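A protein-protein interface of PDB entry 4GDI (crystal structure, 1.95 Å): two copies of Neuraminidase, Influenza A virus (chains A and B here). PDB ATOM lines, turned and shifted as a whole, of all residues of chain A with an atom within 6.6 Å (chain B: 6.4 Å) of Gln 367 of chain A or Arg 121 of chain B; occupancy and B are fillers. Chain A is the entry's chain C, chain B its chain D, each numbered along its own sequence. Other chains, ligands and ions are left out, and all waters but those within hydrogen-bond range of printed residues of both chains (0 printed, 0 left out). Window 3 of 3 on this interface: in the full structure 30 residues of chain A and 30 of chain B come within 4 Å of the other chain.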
ATOM      1  N   TRP A  21      18.201 -19.031  31.036  1.00  0.00           N
ATOM      2  CA  TRP A  21      17.573 -20.137  31.762  1.00  0.00           C
ATOM      3  C   TRP A  21      18.568 -21.248  32.027  1.00  0.00           C
ATOM      4  O   TRP A  21      19.182 -21.763  31.088  1.00  0.00           O
ATOM      5  CB  TRP A  21      16.430 -20.701  30.932  1.00  0.00           C
ATOM      6  CG  TRP A  21      15.409 -19.678  30.575  1.00  0.00           C
ATOM      7  CD1 TRP A  21      15.394 -18.879  29.466  1.00  0.00           C
ATOM      8  CD2 TRP A  21      14.242 -19.342  31.331  1.00  0.00           C
ATOM      9  NE1 TRP A  21      14.285 -18.069  29.486  1.00  0.00           N
ATOM     10  CE2 TRP A  21      13.562 -18.335  30.622  1.00  0.00           C
ATOM     11  CE3 TRP A  21      13.706 -19.797  32.537  1.00  0.00           C
ATOM     12  CZ2 TRP A  21      12.377 -17.769  31.086  1.00  0.00           C
ATOM     13  CZ3 TRP A  21      12.530 -19.241  32.992  1.00  0.00           C
ATOM     14  CH2 TRP A  21      11.877 -18.237  32.270  1.00  0.00           C
ATOM     15  N   TYR A 310      17.593 -19.048  22.847  1.00  0.00           N
ATOM     16  CA  TYR A 310      18.349 -20.136  23.444  1.00  0.00           C
ATOM     17  C   TYR A 310      17.740 -21.472  23.083  1.00  0.00           C
ATOM     18  O   TYR A 310      16.606 -21.758  23.447  1.00  0.00           O
ATOM     19  CB  TYR A 310      18.383 -19.988  24.956  1.00  0.00           C
ATOM     20  CG  TYR A 310      19.248 -18.866  25.451  1.00  0.00           C
ATOM     21  CD1 TYR A 310      20.622 -18.883  25.241  1.00  0.00           C
ATOM     22  CD2 TYR A 310      18.698 -17.793  26.147  1.00  0.00           C
ATOM     23  CE1 TYR A 310      21.425 -17.860  25.699  1.00  0.00           C
ATOM     24  CE2 TYR A 310      19.495 -16.766  26.616  1.00  0.00           C
ATOM     25  CZ  TYR A 310      20.858 -16.805  26.386  1.00  0.00           C
ATOM     26  OH  TYR A 310      21.660 -15.785  26.843  1.00  0.00           O
ATOM     27  N   LEU A 312      17.663 -24.822  24.182  1.00  0.00           N
ATOM     28  CA  LEU A 312      18.014 -25.616  25.357  1.00  0.00           C
ATOM     29  C   LEU A 312      18.202 -27.092  24.988  1.00  0.00           C
ATOM     30  O   LEU A 312      19.103 -27.756  25.498  1.00  0.00           O
ATOM     31  CB  LEU A 312      16.944 -25.464  26.449  1.00  0.00           C
ATOM     32  CG  LEU A 312      16.802 -24.064  27.057  1.00  0.00           C
ATOM     33  CD1 LEU A 312      15.738 -24.054  28.154  1.00  0.00           C
ATOM     34  CD2 LEU A 312      18.134 -23.543  27.610  1.00  0.00           C
ATOM     35  N   PRO A 365      25.082 -13.903  33.843  1.00  0.00           N
ATOM     36  CA  PRO A 365      25.355 -14.319  32.462  1.00  0.00           C
ATOM     37  C   PRO A 365      25.143 -15.811  32.227  1.00  0.00           C
ATOM     38  O   PRO A 365      25.246 -16.612  33.166  1.00  0.00           O
ATOM     39  CB  PRO A 365      26.834 -13.944  32.258  1.00  0.00           C
ATOM     40  CG  PRO A 365      27.435 -13.828  33.647  1.00  0.00           C
ATOM     41  CD  PRO A 365      26.307 -13.857  34.665  1.00  0.00           C
ATOM     42  N   VAL A 366      24.840 -16.183  30.986  1.00  0.00           N
ATOM     43  CA  VAL A 366      24.821 -17.596  30.628  1.00  0.00           C
ATOM     44  C   VAL A 366      25.066 -17.811  29.146  1.00  0.00           C
ATOM     45  O   VAL A 366      24.690 -16.989  28.314  1.00  0.00           O
ATOM     46  CB  VAL A 366      23.499 -18.277  31.023  1.00  0.00           C
ATOM     47  CG1 VAL A 366      22.359 -17.815  30.117  1.00  0.00           C
ATOM     48  CG2 VAL A 366      23.655 -19.795  30.973  1.00  0.00           C
ATOM     49  N   GLN A 367      25.689 -18.943  28.842  1.00  0.00           N
ATOM     50  CA  GLN A 367      26.010 -19.327  27.477  1.00  0.00           C
ATOM     51  C   GLN A 367      24.844 -20.061  26.840  1.00  0.00           C
ATOM     52  O   GLN A 367      23.909 -20.463  27.538  1.00  0.00           O
ATOM     53  CB  GLN A 367      27.248 -20.225  27.475  1.00  0.00           C
ATOM     54  CG  GLN A 367      28.511 -19.537  27.971  1.00  0.00           C
ATOM     55  CD  GLN A 367      28.915 -18.371  27.088  1.00  0.00           C
ATOM     56  OE1 GLN A 367      28.189 -17.994  26.171  1.00  0.00           O
ATOM     57  NE2 GLN A 367      30.078 -17.795  27.360  1.00  0.00           N
ATOM     58  N   ASN A 368      24.912 -20.238  25.521  1.00  0.00           N
ATOM     59  CA  ASN A 368      23.877 -20.955  24.766  1.00  0.00           C
ATOM     60  C   ASN A 368      24.146 -22.455  24.668  1.00  0.00           C
ATOM     61  O   ASN A 368      24.228 -23.006  23.568  1.00  0.00           O
ATOM     62  CB  ASN A 368      23.769 -20.378  23.351  1.00  0.00           C
ATOM     63  CG  ASN A 368      22.517 -20.837  22.621  1.00  0.00           C
ATOM     64  OD1 ASN A 368      21.634 -21.464  23.207  1.00  0.00           O
ATOM     65  ND2 ASN A 368      22.429 -20.510  21.336  1.00  0.00           N
ATOM     66  N   ILE A 369      24.285 -23.105  25.824  1.00  0.00           N
ATOM     67  CA  ILE A 369      24.576 -24.537  25.898  1.00  0.00           C
ATOM     68  C   ILE A 369      23.387 -25.380  25.450  1.00  0.00           C
ATOM     69  O   ILE A 369      22.247 -25.089  25.806  1.00  0.00           O
ATOM     70  CB  ILE A 369      24.934 -24.959  27.343  1.00  0.00           C
ATOM     71  CG1 ILE A 369      26.368 -24.574  27.685  1.00  0.00           C
ATOM     72  CG2 ILE A 369      24.773 -26.455  27.529  1.00  0.00           C
ATOM     73  CD1 ILE A 369      27.411 -25.387  26.931  1.00  0.00           C
ATOM     74  N   TRP A 371      21.640 -28.925  25.964  1.00  0.00           N
ATOM     75  CA  TRP A 371      21.631 -29.959  27.002  1.00  0.00           C
ATOM     76  C   TRP A 371      21.187 -31.357  26.518  1.00  0.00           C
ATOM     77  O   TRP A 371      20.771 -32.190  27.322  1.00  0.00           O
ATOM     78  CB  TRP A 371      20.737 -29.503  28.158  1.00  0.00           C
ATOM     79  CG  TRP A 371      21.184 -28.210  28.764  1.00  0.00           C
ATOM     80  CD1 TRP A 371      20.784 -26.959  28.407  1.00  0.00           C
ATOM     81  CD2 TRP A 371      22.134 -28.041  29.824  1.00  0.00           C
ATOM     82  NE1 TRP A 371      21.419 -26.021  29.182  1.00  0.00           N
ATOM     83  CE2 TRP A 371      22.258 -26.660  30.055  1.00  0.00           C
ATOM     84  CE3 TRP A 371      22.888 -28.924  30.598  1.00  0.00           C
ATOM     85  CZ2 TRP A 371      23.104 -26.139  31.031  1.00  0.00           C
ATOM     86  CZ3 TRP A 371      23.721 -28.407  31.565  1.00  0.00           C
ATOM     87  CH2 TRP A 371      23.824 -27.029  31.775  1.00  0.00           C
ATOM     88  N   ARG B 119      30.760 -27.608  27.280  1.00  0.00           N
ATOM     89  CA  ARG B 119      32.024 -27.951  26.640  1.00  0.00           C
ATOM     90  C   ARG B 119      32.741 -26.686  26.193  1.00  0.00           C
ATOM     91  O   ARG B 119      32.115 -25.733  25.713  1.00  0.00           O
ATOM     92  CB  ARG B 119      31.792 -28.865  25.430  1.00  0.00           C
ATOM     93  CG  ARG B 119      31.247 -30.254  25.761  1.00  0.00           C
ATOM     94  CD  ARG B 119      32.182 -31.050  26.668  1.00  0.00           C
ATOM     95  NE  ARG B 119      33.517 -31.205  26.093  1.00  0.00           N
ATOM     96  CZ  ARG B 119      34.491 -31.930  26.636  1.00  0.00           C
ATOM     97  NH1 ARG B 119      34.289 -32.581  27.776  1.00  0.00           N
ATOM     98  NH2 ARG B 119      35.673 -32.008  26.036  1.00  0.00           N
ATOM     99  N   ASP B 120      34.059 -26.686  26.353  1.00  0.00           N
ATOM    100  CA  ASP B 120      34.899 -25.573  25.914  1.00  0.00           C
ATOM    101  C   ASP B 120      34.267 -24.193  26.162  1.00  0.00           C
ATOM    102  O   ASP B 120      33.945 -23.860  27.302  1.00  0.00           O
ATOM    103  CB  ASP B 120      35.321 -25.754  24.445  1.00  0.00           C
ATOM    104  CG  ASP B 120      34.155 -26.065  23.524  1.00  0.00           C
ATOM    105  OD1 ASP B 120      33.521 -25.111  23.027  1.00  0.00           O
ATOM    106  OD2 ASP B 120      33.887 -27.263  23.279  1.00  0.00           O
ATOM    107  N   ARG B 121      34.091 -23.394  25.112  1.00  0.00           N
ATOM    108  CA  ARG B 121      33.771 -21.974  25.279  1.00  0.00           C
ATOM    109  C   ARG B 121      32.413 -21.698  25.911  1.00  0.00           C
ATOM    110  O   ARG B 121      32.199 -20.620  26.470  1.00  0.00           O
ATOM    111  CB  ARG B 121      33.827 -21.245  23.934  1.00  0.00           C
ATOM    112  CG  ARG B 121      35.208 -20.774  23.521  1.00  0.00           C
ATOM    113  CD  ARG B 121      35.115 -19.752  22.392  1.00  0.00           C
ATOM    114  NE  ARG B 121      34.506 -20.307  21.181  1.00  0.00           N
ATOM    115  CZ  ARG B 121      35.178 -20.699  20.099  1.00  0.00           C
ATOM    116  NH1 ARG B 121      36.503 -20.603  20.042  1.00  0.00           N
ATOM    117  NH2 ARG B 121      34.517 -21.190  19.056  1.00  0.00           N
ATOM    118  N   ASN B 122      31.490 -22.644  25.810  1.00  0.00           N
ATOM    119  CA  ASN B 122      30.161 -22.437  26.375  1.00  0.00           C
ATOM    120  C   ASN B 122      30.076 -22.885  27.830  1.00  0.00           C
ATOM    121  O   ASN B 122      28.995 -22.939  28.410  1.00  0.00           O
ATOM    122  CB  ASN B 122      29.111 -23.161  25.539  1.00  0.00           C
ATOM    123  CG  ASN B 122      28.824 -22.450  24.235  1.00  0.00           C
ATOM    124  OD1 ASN B 122      28.721 -21.219  24.191  1.00  0.00           O
ATOM    125  ND2 ASN B 122      28.697 -23.219  23.162  1.00  0.00           N
ATOM    126  N   SER B 123      31.221 -23.201  28.420  1.00  0.00           N
ATOM    127  CA  SER B 123      31.248 -23.681  29.794  1.00  0.00           C
ATOM    128  C   SER B 123      30.879 -22.559  30.760  1.00  0.00           C
ATOM    129  O   SER B 123      31.283 -21.402  30.579  1.00  0.00           O
ATOM    130  CB  SER B 123      32.637 -24.233  30.128  1.00  0.00           C
ATOM    131  OG  SER B 123      32.650 -24.864  31.401  1.00  0.00           O
ATOM    132  N   PHE B 124      30.102 -22.899  31.785  1.00  0.00           N
ATOM    133  CA  PHE B 124      29.692 -21.921  32.783  1.00  0.00           C
ATOM    134  C   PHE B 124      29.559 -22.558  34.166  1.00  0.00           C
ATOM    135  O   PHE B 124      29.300 -23.751  34.293  1.00  0.00           O
ATOM    136  CB  PHE B 124      28.377 -21.234  32.372  1.00  0.00           C
ATOM    137  CG  PHE B 124      27.142 -22.046  32.624  1.00  0.00           C
ATOM    138  CD1 PHE B 124      26.739 -23.034  31.734  1.00  0.00           C
ATOM    139  CD2 PHE B 124      26.355 -21.798  33.737  1.00  0.00           C
ATOM    140  CE1 PHE B 124      25.598 -23.770  31.962  1.00  0.00           C
ATOM    141  CE2 PHE B 124      25.206 -22.535  33.969  1.00  0.00           C
ATOM    142  CZ  PHE B 124      24.828 -23.520  33.083  1.00  0.00           C
ATOM    143  N   SER B 138      30.809 -17.241  33.349  1.00  0.00           N
ATOM    144  CA  SER B 138      31.208 -17.950  32.145  1.00  0.00           C
ATOM    145  C   SER B 138      32.714 -18.010  32.014  1.00  0.00           C
ATOM    146  O   SER B 138      33.443 -17.203  32.597  1.00  0.00           O
ATOM    147  CB  SER B 138      30.638 -17.250  30.912  1.00  0.00           C
ATOM    148  OG  SER B 138      29.233 -17.408  30.836  1.00  0.00           O
ATOM    149  N   ALA B 139      33.161 -18.976  31.226  1.00  0.00           N
ATOM    150  CA  ALA B 139      34.563 -19.136  30.905  1.00  0.00           C
ATOM    151  C   ALA B 139      35.072 -17.849  30.278  1.00  0.00           C
ATOM    152  O   ALA B 139      34.371 -17.200  29.503  1.00  0.00           O
ATOM    153  CB  ALA B 139      34.741 -20.299  29.948  1.00  0.00           C
ATOM    154  N   ARG B 141      38.623 -17.789  29.311  1.00  0.00           N
ATOM    155  CA  ARG B 141      39.836 -18.128  28.583  1.00  0.00           C
ATOM    156  C   ARG B 141      39.668 -19.374  27.721  1.00  0.00           C
ATOM    157  O   ARG B 141      40.605 -20.151  27.551  1.00  0.00           O
ATOM    158  CB  ARG B 141      40.999 -18.293  29.560  1.00  0.00           C
ATOM    159  CG  ARG B 141      41.278 -17.030  30.368  1.00  0.00           C
ATOM    160  CD  ARG B 141      41.899 -15.926  29.501  1.00  0.00           C
ATOM    161  NE  ARG B 141      43.302 -16.209  29.195  1.00  0.00           N
ATOM    162  CZ  ARG B 141      44.342 -15.727  29.877  1.00  0.00           C
ATOM    163  NH1 ARG B 141      44.162 -14.910  30.910  1.00  0.00           N
ATOM    164  NH2 ARG B 141      45.577 -16.055  29.517  1.00  0.00           N
ATOM    165  N   GLY B 142      38.473 -19.557  27.172  1.00  0.00           N
ATOM    166  CA  GLY B 142      38.247 -20.623  26.209  1.00  0.00           C
ATOM    167  C   GLY B 142      37.591 -21.871  26.769  1.00  0.00           C
ATOM    168  O   GLY B 142      37.083 -22.691  26.013  1.00  0.00           O
ATOM    169  N   GLY B 143      37.600 -22.024  28.092  1.00  0.00           N
ATOM    170  CA  GLY B 143      36.988 -23.180  28.721  1.00  0.00           C
ATOM    171  C   GLY B 143      37.803 -24.451  28.556  1.00  0.00           C
ATOM    172  O   GLY B 143      38.846 -24.439  27.911  1.00  0.00           O
ATOM    173  N   PRO B 144      37.346 -25.553  29.171  1.00  0.00           N
ATOM    174  CA  PRO B 144      36.166 -25.558  30.040  1.00  0.00           C
ATOM    175  C   PRO B 144      36.494 -24.981  31.420  1.00  0.00           C
ATOM    176  O   PRO B 144      37.662 -24.968  31.831  1.00  0.00           O
ATOM    177  CB  PRO B 144      35.847 -27.046  30.160  1.00  0.00           C
ATOM    178  CG  PRO B 144      37.204 -27.683  30.154  1.00  0.00           C
ATOM    179  CD  PRO B 144      38.035 -26.856  29.184  1.00  0.00           C
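Gln 367 of chain A touches just these residues of chain B: Arg 121, Asn 122 and Ser 138.
Printed residues of chain B within 4 Å of Ile 369 of chain A: Asn 122 (3.1 Å).
Printed residues of chain B within 4 Å of Trp 371 of chain A: Phe 124.
Arg 121 of chain B touches just one residue of chain A: Gln 367.
Of the printed residues of chain A, Asn 122 of chain B touches Gln 367 (3.4 Å) and Ile 369 (3.1 Å).
The nearest residue of chain B that does not touch Gln 367 of chain A is Ser 123 of chain B (4.2 Å).
The backbone NH of Arg 121 of chain B lies within hydrogen-bond range of the backbone carbonyl oxygen of Gly 142 of chain B (3.2 Å).
The backbone NH (N) of Trp 371 of chain A lies within hydrogen-bond range of the backbone carbonyl oxygen (O) of Leu 312 of chain A (2.8 Å).
Of the 12 printed residues of chain B, 4 touch a printed residue of chain A.
Hydrophobic or aromatic side chains of chain B within 4 Å of the printed part of chain A: Phe 124.
Of the 9 printed residues of chain A, 3 touch a printed residue of chain B.
Hydrophobic or aromatic side chains of chain A within 4 Å of the printed part of chain B: Ile 369 and Trp 371.
Along chain A the printed residues that touch a printed residue of chain B span positions 367 to 371.
Among the printed residues, 5 pairs touch across the chains.
O of Arg 121 of chain B touches NE2 of Gln 367 of chain A (3.6 Å).
CB of Gln 367 of chain A touches O of Asn 122 of chain B, at 3.4 Å.
Gln 367 of chain A touches Ser 138 of chain B (NE2 to OG, 3.6 Å).
CB of Asn 122 of chain B touches CD1 of Ile 369 of chain A, 3.1 Å away.
Phe 124 of chain B touches Trp 371 of chain A (CE1 to CZ2, 3.6 Å).
No position is printed for both chains.
Of the 5 pairs that touch across the chains among the printed residues, none has its exchanged pair printed and touching as well.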
